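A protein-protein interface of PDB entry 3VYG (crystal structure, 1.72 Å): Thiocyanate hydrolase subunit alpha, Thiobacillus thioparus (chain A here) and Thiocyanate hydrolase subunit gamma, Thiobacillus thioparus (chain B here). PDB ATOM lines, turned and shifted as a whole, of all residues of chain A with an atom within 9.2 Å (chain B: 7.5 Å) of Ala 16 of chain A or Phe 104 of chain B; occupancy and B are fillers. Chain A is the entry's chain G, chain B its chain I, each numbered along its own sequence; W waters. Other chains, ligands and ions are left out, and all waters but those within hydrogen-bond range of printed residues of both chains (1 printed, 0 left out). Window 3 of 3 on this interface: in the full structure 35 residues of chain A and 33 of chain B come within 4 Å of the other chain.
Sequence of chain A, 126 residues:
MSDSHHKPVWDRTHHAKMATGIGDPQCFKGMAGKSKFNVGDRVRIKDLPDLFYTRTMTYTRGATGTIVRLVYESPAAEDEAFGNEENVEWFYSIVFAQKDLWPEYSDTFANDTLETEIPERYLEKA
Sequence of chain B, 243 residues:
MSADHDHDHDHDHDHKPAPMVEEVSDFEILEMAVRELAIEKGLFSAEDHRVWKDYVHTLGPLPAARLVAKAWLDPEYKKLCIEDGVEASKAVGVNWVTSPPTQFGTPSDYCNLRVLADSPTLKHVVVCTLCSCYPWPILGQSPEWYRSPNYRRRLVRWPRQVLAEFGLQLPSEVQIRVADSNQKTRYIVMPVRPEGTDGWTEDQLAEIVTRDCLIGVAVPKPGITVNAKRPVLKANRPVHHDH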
ATOM      1  N   ASP A  11      16.580  23.057  17.755  1.00  0.00           N
ATOM      2  CA  ASP A  11      17.527  23.714  16.834  1.00  0.00           C
ATOM      3  C   ASP A  11      16.937  23.742  15.439  1.00  0.00           C
ATOM      4  O   ASP A  11      16.910  22.707  14.730  1.00  0.00           O
ATOM      5  CB  ASP A  11      18.795  22.898  16.833  1.00  0.00           C
ATOM      6  CG  ASP A  11      19.838  23.416  15.876  1.00  0.00           C
ATOM      7  OD1 ASP A  11      19.619  24.315  14.999  1.00  0.00           O
ATOM      8  OD2 ASP A  11      20.926  22.902  16.080  1.00  0.00           O
ATOM      9  N   ARG A  12      16.534  24.936  15.008  1.00  0.00           N
ATOM     10  CA  ARG A  12      15.885  25.071  13.726  1.00  0.00           C
ATOM     11  C   ARG A  12      16.886  25.253  12.562  1.00  0.00           C
ATOM     12  O   ARG A  12      16.466  25.314  11.405  1.00  0.00           O
ATOM     13  CB  ARG A  12      14.852  26.199  13.773  1.00  0.00           C
ATOM     14  CG  ARG A  12      13.684  25.733  14.662  1.00  0.00           C
ATOM     15  CD  ARG A  12      12.938  26.773  15.400  1.00  0.00           C
ATOM     16  NE  ARG A  12      12.599  27.894  14.606  1.00  0.00           N
ATOM     17  CZ  ARG A  12      12.467  29.125  15.093  1.00  0.00           C
ATOM     18  NH1 ARG A  12      12.158  30.096  14.240  1.00  0.00           N
ATOM     19  NH2 ARG A  12      12.637  29.407  16.407  1.00  0.00           N
ATOM     20  N   THR A  13      18.190  25.345  12.862  1.00  0.00           N
ATOM     21  CA  THR A  13      19.122  25.576  11.744  1.00  0.00           C
ATOM     22  C   THR A  13      19.869  24.389  11.356  1.00  0.00           C
ATOM     23  O   THR A  13      20.578  24.394  10.323  1.00  0.00           O
ATOM     24  CB  THR A  13      20.169  26.704  12.094  1.00  0.00           C
ATOM     25  OG1 THR A  13      20.942  26.293  13.235  1.00  0.00           O
ATOM     26  CG2 THR A  13      19.468  27.965  12.367  1.00  0.00           C
ATOM     27  N   HIS A  14      19.774  23.313  12.149  1.00  0.00           N
ATOM     28  CA  HIS A  14      20.732  22.213  11.922  1.00  0.00           C
ATOM     29  C   HIS A  14      20.610  21.555  10.525  1.00  0.00           C
ATOM     30  O   HIS A  14      21.622  21.239   9.809  1.00  0.00           O
ATOM     31  CB  HIS A  14      20.547  21.121  12.989  1.00  0.00           C
ATOM     32  CG  HIS A  14      21.238  19.828  12.654  1.00  0.00           C
ATOM     33  ND1 HIS A  14      22.592  19.620  12.849  1.00  0.00           N
ATOM     34  CD2 HIS A  14      20.761  18.684  12.107  1.00  0.00           C
ATOM     35  CE1 HIS A  14      22.908  18.395  12.449  1.00  0.00           C
ATOM     36  NE2 HIS A  14      21.817  17.814  11.973  1.00  0.00           N
ATOM     37  N   HIS A  15      19.361  21.237  10.126  1.00  0.00           N
ATOM     38  CA  HIS A  15      19.209  20.570   8.832  1.00  0.00           C
ATOM     39  C   HIS A  15      19.654  21.478   7.643  1.00  0.00           C
ATOM     40  O   HIS A  15      20.322  20.966   6.766  1.00  0.00           O
ATOM     41  CB  HIS A  15      17.748  20.156   8.633  1.00  0.00           C
ATOM     42  CG  HIS A  15      17.515  19.338   7.418  1.00  0.00           C
ATOM     43  ND1 HIS A  15      17.952  18.020   7.308  1.00  0.00           N
ATOM     44  CD2 HIS A  15      16.871  19.627   6.269  1.00  0.00           C
ATOM     45  CE1 HIS A  15      17.619  17.551   6.110  1.00  0.00           C
ATOM     46  NE2 HIS A  15      16.924  18.486   5.480  1.00  0.00           N
ATOM     47  N   ALA A  16      19.236  22.728   7.628  1.00  0.00           N
ATOM     48  CA  ALA A  16      19.690  23.655   6.544  1.00  0.00           C
ATOM     49  C   ALA A  16      21.227  23.803   6.546  1.00  0.00           C
ATOM     50  O   ALA A  16      21.842  23.834   5.453  1.00  0.00           O
ATOM     51  CB  ALA A  16      19.007  25.027   6.589  1.00  0.00           C
ATOM     52  N   LYS A  17      21.881  23.857   7.704  1.00  0.00           N
ATOM     53  CA  LYS A  17      23.366  23.966   7.739  1.00  0.00           C
ATOM     54  C   LYS A  17      24.026  22.762   7.134  1.00  0.00           C
ATOM     55  O   LYS A  17      24.997  22.895   6.353  1.00  0.00           O
ATOM     56  CB  LYS A  17      23.920  24.254   9.177  1.00  0.00           C
ATOM     57  CG  LYS A  17      23.608  25.726   9.600  1.00  0.00           C
ATOM     58  N   MET A  18      23.473  21.563   7.389  1.00  0.00           N
ATOM     59  CA  MET A  18      24.053  20.315   6.896  1.00  0.00           C
ATOM     60  C   MET A  18      23.728  20.086   5.419  1.00  0.00           C
ATOM     61  O   MET A  18      24.552  19.528   4.671  1.00  0.00           O
ATOM     62  CB  MET A  18      23.382  19.149   7.746  1.00  0.00           C
ATOM     63  CG  MET A  18      23.298  17.822   7.055  1.00  0.00           C
ATOM     64  SD  MET A  18      23.135  16.652   8.440  1.00  0.00           S
ATOM     65  CE  MET A  18      24.284  15.381   7.882  1.00  0.00           C
ATOM     66  N   ALA A  19      22.527  20.524   4.972  1.00  0.00           N
ATOM     67  CA  ALA A  19      22.064  20.058   3.642  1.00  0.00           C
ATOM     68  C   ALA A  19      22.211  21.080   2.529  1.00  0.00           C
ATOM     69  O   ALA A  19      22.220  20.690   1.362  1.00  0.00           O
ATOM     70  CB  ALA A  19      20.604  19.628   3.684  1.00  0.00           C
ATOM     71  N   THR A  20      22.275  22.354   2.904  1.00  0.00           N
ATOM     72  CA  THR A  20      22.256  23.434   1.866  1.00  0.00           C
ATOM     73  C   THR A  20      23.441  23.259   0.906  1.00  0.00           C
ATOM     74  O   THR A  20      24.616  23.011   1.334  1.00  0.00           O
ATOM     75  CB  THR A  20      22.325  24.849   2.515  1.00  0.00           C
ATOM     76  OG1 THR A  20      21.102  25.107   3.197  1.00  0.00           O
ATOM     77  CG2 THR A  20      22.378  25.880   1.386  1.00  0.00           C
ATOM     78  N   GLY A  21      23.095  23.281  -0.406  1.00  0.00           N
ATOM     79  CA  GLY A  21      24.059  22.989  -1.476  1.00  0.00           C
ATOM     80  C   GLY A  21      24.543  21.581  -1.691  1.00  0.00           C
ATOM     81  O   GLY A  21      25.360  21.349  -2.556  1.00  0.00           O
ATOM     82  N   ILE A  22      23.976  20.632  -0.942  1.00  0.00           N
ATOM     83  CA  ILE A  22      24.427  19.292  -0.967  1.00  0.00           C
ATOM     84  C   ILE A  22      23.178  18.458  -1.390  1.00  0.00           C
ATOM     85  O   ILE A  22      23.132  17.776  -2.414  1.00  0.00           O
ATOM     86  CB  ILE A  22      24.931  18.937   0.477  1.00  0.00           C
ATOM     87  CG1 ILE A  22      26.122  19.838   0.842  1.00  0.00           C
ATOM     88  CG2 ILE A  22      25.407  17.510   0.534  1.00  0.00           C
ATOM     89  CD1 ILE A  22      27.274  19.380   0.005  1.00  0.00           C
ATOM     90  N   GLY A  23      22.171  18.585  -0.546  1.00  0.00           N
ATOM     91  CA  GLY A  23      20.855  17.877  -0.730  1.00  0.00           C
ATOM     92  C   GLY A  23      20.725  16.739   0.272  1.00  0.00           C
ATOM     93  O   GLY A  23      21.660  16.356   0.972  1.00  0.00           O
ATOM     94  N   ASP A  24      19.509  16.151   0.287  1.00  0.00           N
ATOM     95  CA  ASP A  24      19.192  15.062   1.209  1.00  0.00           C
ATOM     96  C   ASP A  24      18.664  13.955   0.220  1.00  0.00           C
ATOM     97  O   ASP A  24      17.777  14.236  -0.511  1.00  0.00           O
ATOM     98  CB  ASP A  24      18.033  15.579   2.076  1.00  0.00           C
ATOM     99  CG  ASP A  24      17.510  14.544   3.069  1.00  0.00           C
ATOM    100  OD1 ASP A  24      17.935  13.378   2.969  1.00  0.00           O
ATOM    101  OD2 ASP A  24      16.611  14.960   3.932  1.00  0.00           O
ATOM    102  N   PRO A  25      19.271  12.775   0.144  1.00  0.00           N
ATOM    103  CA  PRO A  25      20.193  12.209   1.137  1.00  0.00           C
ATOM    104  C   PRO A  25      21.709  12.330   0.900  1.00  0.00           C
ATOM    105  O   PRO A  25      22.485  11.741   1.660  1.00  0.00           O
ATOM    106  CB  PRO A  25      19.791  10.783   1.173  1.00  0.00           C
ATOM    107  CG  PRO A  25      19.403  10.471  -0.297  1.00  0.00           C
ATOM    108  CD  PRO A  25      18.710  11.734  -0.785  1.00  0.00           C
ATOM    109  N   GLN A  26      22.064  13.176  -0.072  1.00  0.00           N
ATOM    110  CA  GLN A  26      23.513  13.369  -0.318  1.00  0.00           C
ATOM    111  C   GLN A  26      24.282  13.774   0.939  1.00  0.00           C
ATOM    112  O   GLN A  26      25.527  13.485   1.022  1.00  0.00           O
ATOM    113  CB  GLN A  26      23.708  14.487  -1.377  1.00  0.00           C
ATOM    114  CG  GLN A  26      23.350  14.052  -2.809  1.00  0.00           C
ATOM    115  CD  GLN A  26      21.876  14.169  -3.241  1.00  0.00           C
ATOM    116  OE1 GLN A  26      21.575  14.161  -4.480  1.00  0.00           O
ATOM    117  NE2 GLN A  26      20.983  14.341  -2.292  1.00  0.00           N
ATOM    118  N   CYS A  27      23.641  14.473   1.861  1.00  0.00           N
ATOM    119  CA  CYS A  27      24.296  15.029   3.012  1.00  0.00           C
ATOM    120  C   CYS A  27      24.721  13.960   4.019  1.00  0.00           C
ATOM    121  O   CYS A  27      25.585  14.208   4.873  1.00  0.00           O
ATOM    122  CB  CYS A  27      23.512  16.153   3.673  1.00  0.00           C
ATOM    123  SG  CYS A  27      21.883  15.545   4.239  1.00  0.00           S
ATOM    124  N   GLU A  85      18.991  11.576  14.201  1.00  0.00           N
ATOM    125  CA  GLU A  85      19.625  11.339  12.889  1.00  0.00           C
ATOM    126  C   GLU A  85      21.114  10.994  13.110  1.00  0.00           C
ATOM    127  O   GLU A  85      21.899  11.090  12.178  1.00  0.00           O
ATOM    128  CB  GLU A  85      19.525  12.662  12.109  1.00  0.00           C
ATOM    129  CG  GLU A  85      18.102  13.000  11.604  1.00  0.00           C
ATOM    130  CD  GLU A  85      18.005  14.342  10.896  1.00  0.00           C
ATOM    131  OE1 GLU A  85      19.085  14.960  10.623  1.00  0.00           O
ATOM    132  OE2 GLU A  85      16.856  14.788  10.587  1.00  0.00           O
ATOM    133  N   TRP B  52       7.266  30.015  -1.788  1.00  0.00           N
ATOM    134  CA  TRP B  52       7.043  28.569  -1.946  1.00  0.00           C
ATOM    135  C   TRP B  52       5.875  28.399  -2.886  1.00  0.00           C
ATOM    136  O   TRP B  52       5.939  27.550  -3.797  1.00  0.00           O
ATOM    137  CB  TRP B  52       6.755  27.828  -0.574  1.00  0.00           C
ATOM    138  CG  TRP B  52       7.012  26.401  -0.829  1.00  0.00           C
ATOM    139  CD1 TRP B  52       6.109  25.440  -1.331  1.00  0.00           C
ATOM    140  CD2 TRP B  52       8.282  25.770  -0.800  1.00  0.00           C
ATOM    141  NE1 TRP B  52       6.805  24.258  -1.554  1.00  0.00           N
ATOM    142  CE2 TRP B  52       8.108  24.424  -1.194  1.00  0.00           C
ATOM    143  CE3 TRP B  52       9.576  26.206  -0.388  1.00  0.00           C
ATOM    144  CZ2 TRP B  52       9.190  23.494  -1.238  1.00  0.00           C
ATOM    145  CZ3 TRP B  52      10.610  25.259  -0.379  1.00  0.00           C
ATOM    146  CH2 TRP B  52      10.398  23.934  -0.789  1.00  0.00           C
ATOM    147  N   TRP B  96      17.678  18.940  -8.739  1.00  0.00           N
ATOM    148  CA  TRP B  96      16.855  18.639  -7.548  1.00  0.00           C
ATOM    149  C   TRP B  96      17.385  19.271  -6.264  1.00  0.00           C
ATOM    150  O   TRP B  96      16.584  19.418  -5.300  1.00  0.00           O
ATOM    151  CB  TRP B  96      16.825  17.074  -7.407  1.00  0.00           C
ATOM    152  CG  TRP B  96      15.946  16.519  -8.390  1.00  0.00           C
ATOM    153  CD1 TRP B  96      16.033  16.631  -9.812  1.00  0.00           C
ATOM    154  CD2 TRP B  96      14.722  15.795  -8.124  1.00  0.00           C
ATOM    155  NE1 TRP B  96      14.929  16.026 -10.400  1.00  0.00           N
ATOM    156  CE2 TRP B  96      14.111  15.528  -9.393  1.00  0.00           C
ATOM    157  CE3 TRP B  96      14.103  15.384  -6.937  1.00  0.00           C
ATOM    158  CZ2 TRP B  96      12.925  14.822  -9.523  1.00  0.00           C
ATOM    159  CZ3 TRP B  96      12.882  14.674  -7.059  1.00  0.00           C
ATOM    160  CH2 TRP B  96      12.315  14.428  -8.315  1.00  0.00           C
ATOM    161  N   VAL B  97      18.673  19.627  -6.213  1.00  0.00           N
ATOM    162  CA  VAL B  97      19.218  20.347  -5.021  1.00  0.00           C
ATOM    163  C   VAL B  97      18.864  21.821  -5.127  1.00  0.00           C
ATOM    164  O   VAL B  97      18.373  22.438  -4.191  1.00  0.00           O
ATOM    165  CB  VAL B  97      20.742  20.088  -4.891  1.00  0.00           C
ATOM    166  CG1 VAL B  97      21.393  20.833  -3.675  1.00  0.00           C
ATOM    167  CG2 VAL B  97      20.999  18.593  -4.828  1.00  0.00           C
ATOM    168  N   THR B  98      19.254  22.428  -6.244  1.00  0.00           N
ATOM    169  CA  THR B  98      19.291  23.894  -6.243  1.00  0.00           C
ATOM    170  C   THR B  98      18.112  24.575  -6.871  1.00  0.00           C
ATOM    171  O   THR B  98      18.020  25.836  -6.775  1.00  0.00           O
ATOM    172  CB  THR B  98      20.634  24.425  -6.908  1.00  0.00           C
ATOM    173  OG1 THR B  98      20.627  23.908  -8.247  1.00  0.00           O
ATOM    174  CG2 THR B  98      21.809  23.907  -6.142  1.00  0.00           C
ATOM    175  N   SER B  99      17.195  23.848  -7.563  1.00  0.00           N
ATOM    176  CA  SER B  99      16.019  24.489  -8.190  1.00  0.00           C
ATOM    177  C   SER B  99      14.951  24.987  -7.197  1.00  0.00           C
ATOM    178  O   SER B  99      14.393  26.070  -7.340  1.00  0.00           O
ATOM    179  CB  SER B  99      15.387  23.670  -9.307  1.00  0.00           C
ATOM    180  OG  SER B  99      16.259  23.496 -10.430  1.00  0.00           O
ATOM    181  N   PRO B 100      14.705  24.224  -6.118  1.00  0.00           N
ATOM    182  CA  PRO B 100      13.739  24.662  -5.095  1.00  0.00           C
ATOM    183  C   PRO B 100      14.277  25.722  -4.138  1.00  0.00           C
ATOM    184  O   PRO B 100      15.473  25.802  -3.955  1.00  0.00           O
ATOM    185  CB  PRO B 100      13.510  23.433  -4.208  1.00  0.00           C
ATOM    186  CG  PRO B 100      14.236  22.318  -4.870  1.00  0.00           C
ATOM    187  CD  PRO B 100      15.299  22.897  -5.825  1.00  0.00           C
ATOM    188  N   PRO B 101      13.362  26.457  -3.492  1.00  0.00           N
ATOM    189  CA  PRO B 101      13.848  27.617  -2.724  1.00  0.00           C
ATOM    190  C   PRO B 101      14.778  27.294  -1.574  1.00  0.00           C
ATOM    191  O   PRO B 101      15.570  28.125  -1.152  1.00  0.00           O
ATOM    192  CB  PRO B 101      12.540  28.212  -2.185  1.00  0.00           C
ATOM    193  CG  PRO B 101      11.544  27.890  -3.212  1.00  0.00           C
ATOM    194  CD  PRO B 101      11.903  26.480  -3.646  1.00  0.00           C
ATOM    195  N   THR B 102      14.693  26.075  -0.992  1.00  0.00           N
ATOM    196  CA  THR B 102      15.635  25.698   0.078  1.00  0.00           C
ATOM    197  C   THR B 102      17.136  25.605  -0.248  1.00  0.00           C
ATOM    198  O   THR B 102      17.993  25.644   0.624  1.00  0.00           O
ATOM    199  CB  THR B 102      15.277  24.230   0.505  1.00  0.00           C
ATOM    200  OG1 THR B 102      15.444  23.373  -0.657  1.00  0.00           O
ATOM    201  CG2 THR B 102      13.815  24.169   1.053  1.00  0.00           C
ATOM    202  N   GLN B 103      17.403  25.329  -1.520  1.00  0.00           N
ATOM    203  CA  GLN B 103      18.736  24.954  -2.004  1.00  0.00           C
ATOM    204  C   GLN B 103      19.226  23.693  -1.388  1.00  0.00           C
ATOM    205  O   GLN B 103      20.376  23.449  -1.312  1.00  0.00           O
ATOM    206  CB  GLN B 103      19.785  26.055  -1.669  1.00  0.00           C
ATOM    207  CG  GLN B 103      20.895  26.054  -2.774  1.00  0.00           C
ATOM    208  CD  GLN B 103      21.979  27.075  -2.378  1.00  0.00           C
ATOM    209  OE1 GLN B 103      21.590  28.137  -1.857  1.00  0.00           O
ATOM    210  NE2 GLN B 103      23.302  26.783  -2.603  1.00  0.00           N
ATOM    211  N   PHE B 104      18.289  22.864  -0.932  1.00  0.00           N
ATOM    212  CA  PHE B 104      18.668  21.528  -0.417  1.00  0.00           C
ATOM    213  C   PHE B 104      17.681  20.459  -0.871  1.00  0.00           C
ATOM    214  O   PHE B 104      17.598  19.363  -0.209  1.00  0.00           O
ATOM    215  CB  PHE B 104      18.984  21.434   1.125  1.00  0.00           C
ATOM    216  CG  PHE B 104      17.893  21.903   2.056  1.00  0.00           C
ATOM    217  CD1 PHE B 104      16.747  21.081   2.297  1.00  0.00           C
ATOM    218  CD2 PHE B 104      18.014  23.091   2.725  1.00  0.00           C
ATOM    219  CE1 PHE B 104      15.751  21.479   3.201  1.00  0.00           C
ATOM    220  CE2 PHE B 104      17.060  23.504   3.645  1.00  0.00           C
ATOM    221  CZ  PHE B 104      15.952  22.716   3.908  1.00  0.00           C
ATOM    222  N   GLY B 105      16.985  20.735  -1.963  1.00  0.00           N
ATOM    223  CA  GLY B 105      15.875  19.838  -2.440  1.00  0.00           C
ATOM    224  C   GLY B 105      14.628  20.234  -1.665  1.00  0.00           C
ATOM    225  O   GLY B 105      14.693  20.915  -0.637  1.00  0.00           O
ATOM    226  N   THR B 106      13.479  19.852  -2.186  1.00  0.00           N
ATOM    227  CA  THR B 106      12.280  20.204  -1.391  1.00  0.00           C
ATOM    228  C   THR B 106      12.340  19.267  -0.148  1.00  0.00           C
ATOM    229  O   THR B 106      12.848  18.182  -0.258  1.00  0.00           O
ATOM    230  CB  THR B 106      10.980  19.986  -2.138  1.00  0.00           C
ATOM    231  OG1 THR B 106      10.855  18.590  -2.551  1.00  0.00           O
ATOM    232  CG2 THR B 106      10.895  20.836  -3.404  1.00  0.00           C
ATOM    233  N   PRO B 107      11.787  19.726   0.981  1.00  0.00           N
ATOM    234  CA  PRO B 107      11.819  18.912   2.173  1.00  0.00           C
ATOM    235  C   PRO B 107      11.078  17.578   1.953  1.00  0.00           C
ATOM    236  O   PRO B 107      11.556  16.588   2.526  1.00  0.00           O
ATOM    237  CB  PRO B 107      10.997  19.749   3.156  1.00  0.00           C
ATOM    238  CG  PRO B 107      11.466  21.174   2.822  1.00  0.00           C
ATOM    239  CD  PRO B 107      11.302  21.090   1.290  1.00  0.00           C
ATOM    240  N   SER B 108       9.993  17.569   1.147  1.00  0.00           N
ATOM    241  CA  SER B 108       9.201  16.324   1.028  1.00  0.00           C
ATOM    242  C   SER B 108       9.564  15.431  -0.148  1.00  0.00           C
ATOM    243  O   SER B 108       9.239  14.232  -0.120  1.00  0.00           O
ATOM    244  CB  SER B 108       7.773  16.664   0.842  1.00  0.00           C
ATOM    245  OG  SER B 108       7.407  17.112   2.122  1.00  0.00           O
ATOM    246  N   TYR B 110      12.900  15.317  -1.635  1.00  0.00           N
ATOM    247  CA  TYR B 110      14.336  14.921  -1.512  1.00  0.00           C
ATOM    248  C   TYR B 110      15.082  15.036  -2.879  1.00  0.00           C
ATOM    249  O   TYR B 110      14.619  15.723  -3.812  1.00  0.00           O
ATOM    250  CB  TYR B 110      14.470  13.488  -1.020  1.00  0.00           C
ATOM    251  CG  TYR B 110      13.711  13.333   0.303  1.00  0.00           C
ATOM    252  CD1 TYR B 110      14.177  13.938   1.454  1.00  0.00           C
ATOM    253  CD2 TYR B 110      12.491  12.638   0.329  1.00  0.00           C
ATOM    254  CE1 TYR B 110      13.471  13.779   2.714  1.00  0.00           C
ATOM    255  CE2 TYR B 110      11.775  12.488   1.551  1.00  0.00           C
ATOM    256  CZ  TYR B 110      12.269  13.011   2.720  1.00  0.00           C
ATOM    257  OH  TYR B 110      11.617  12.886   3.946  1.00  0.00           O
ATOM    258  N   CYS B 111      16.216  14.388  -2.949  1.00  0.00           N
ATOM    259  CA  CYS B 111      17.122  14.549  -4.086  1.00  0.00           C
ATOM    260  C   CYS B 111      17.645  13.269  -4.641  1.00  0.00           C
ATOM    261  O   CYS B 111      18.820  13.201  -4.964  1.00  0.00           O
ATOM    262  CB  CYS B 111      18.361  15.447  -3.684  1.00  0.00           C
ATOM    263  SG  CYS B 111      17.876  16.996  -2.874  1.00  0.00           S
HETATM  264  O   HOH W   1      20.752  11.085  -3.666  1.00  0.00           O
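Among the printed residues, 15 pairs touch across the chains. Among the printed residues, no Asp or Glu carboxylate lies within 4 Å of a Lys or Arg side-chain nitrogen of the other chain.
Among the printed residues, merely in contact across the chains: Ile 22 of chain A with Val 97 of chain B (3.3 Å), Ala 19 of chain A with Phe 104 of chain B (3.3 Å), Asp 24 of chain A with Tyr 110 of chain B (3.4 Å), Gly 23 of chain A with Phe 104 of chain B (3.6 Å), Thr 20 of chain A with Gln 103 of chain B (3.7 Å), Thr 20 of chain A with Phe 104 of chain B (3.7 Å), His 15 of chain A with Phe 104 of chain B (3.8 Å), Asp 24 of chain A with Phe 104 of chain B (3.8 Å), Gly 23 of chain A with Cys 111 of chain B (3.8 Å), Gly 21 of chain A with Val 97 of chain B (3.8 Å), Ala 16 of chain A with Phe 104 of chain B (3.8 Å) and Gly 23 of chain A with Val 97 of chain B (3.9 Å).
Water W1 bridges O of Cys 111 of chain B (3.1 Å) and OE1 of Gln 26 of chain A (3.3 Å).
The backbone NH (N) of Gly 21 of chain A is in hydrogen-bond range of the backbone carbonyl oxygen (O) of Gln 103 of chain B (2.9 Å). O of Asp 24 of chain A is in hydrogen-bond range of N of Cys 111 of chain B, at 2.9 Å. OE1 of Gln 26 of chain A sits close to O of Cys 111 of chain B (3.0 Å).
The backbone carbonyl oxygen of Ala 16 of chain A is in hydrogen-bond range of the side-chain hydroxyl of Thr 20 of chain A. The side-chain sulfur of Cys 27 of chain A sits close to the backbone carbonyl oxygen of Gly 23 of chain A, at 3.4 Å. The side-chain sulfur (SG) of Cys 111 of chain B is in hydrogen-bond range of the backbone carbonyl oxygen (O) of Trp 96 of chain B, at 3.7 Å. O of Val 97 of chain B is in hydrogen-bond range of N of Phe 104 of chain B (3.3 Å). N of Gly 105 of chain B lies within hydrogen-bond range of O of Val 97 of chain B, 3.1 Å away. The side-chain hydroxyl of Thr 102 of chain B lies within hydrogen-bond range of the backbone NH of Phe 104 of chain B.
Ala 16 of chain A touches one residue of chain B. Phe 104 of chain B touches six residues of chain A. Thr 102 of chain B touches none of the printed residues of chain A. Printed residues of chain B within 4 Å of His 15 of chain A: Phe 104 (3.8 Å). Of the printed residues of chain B, Thr 20 of chain A touches Gln 103 and Phe 104. Ser 99 of chain B touches none of the printed residues of chain A. Met 18 of chain A touches none of the printed residues of chain B. The nearest printed residue of chain B that does not touch His 15 of chain A is Pro 107 of chain B (6.1 Å).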
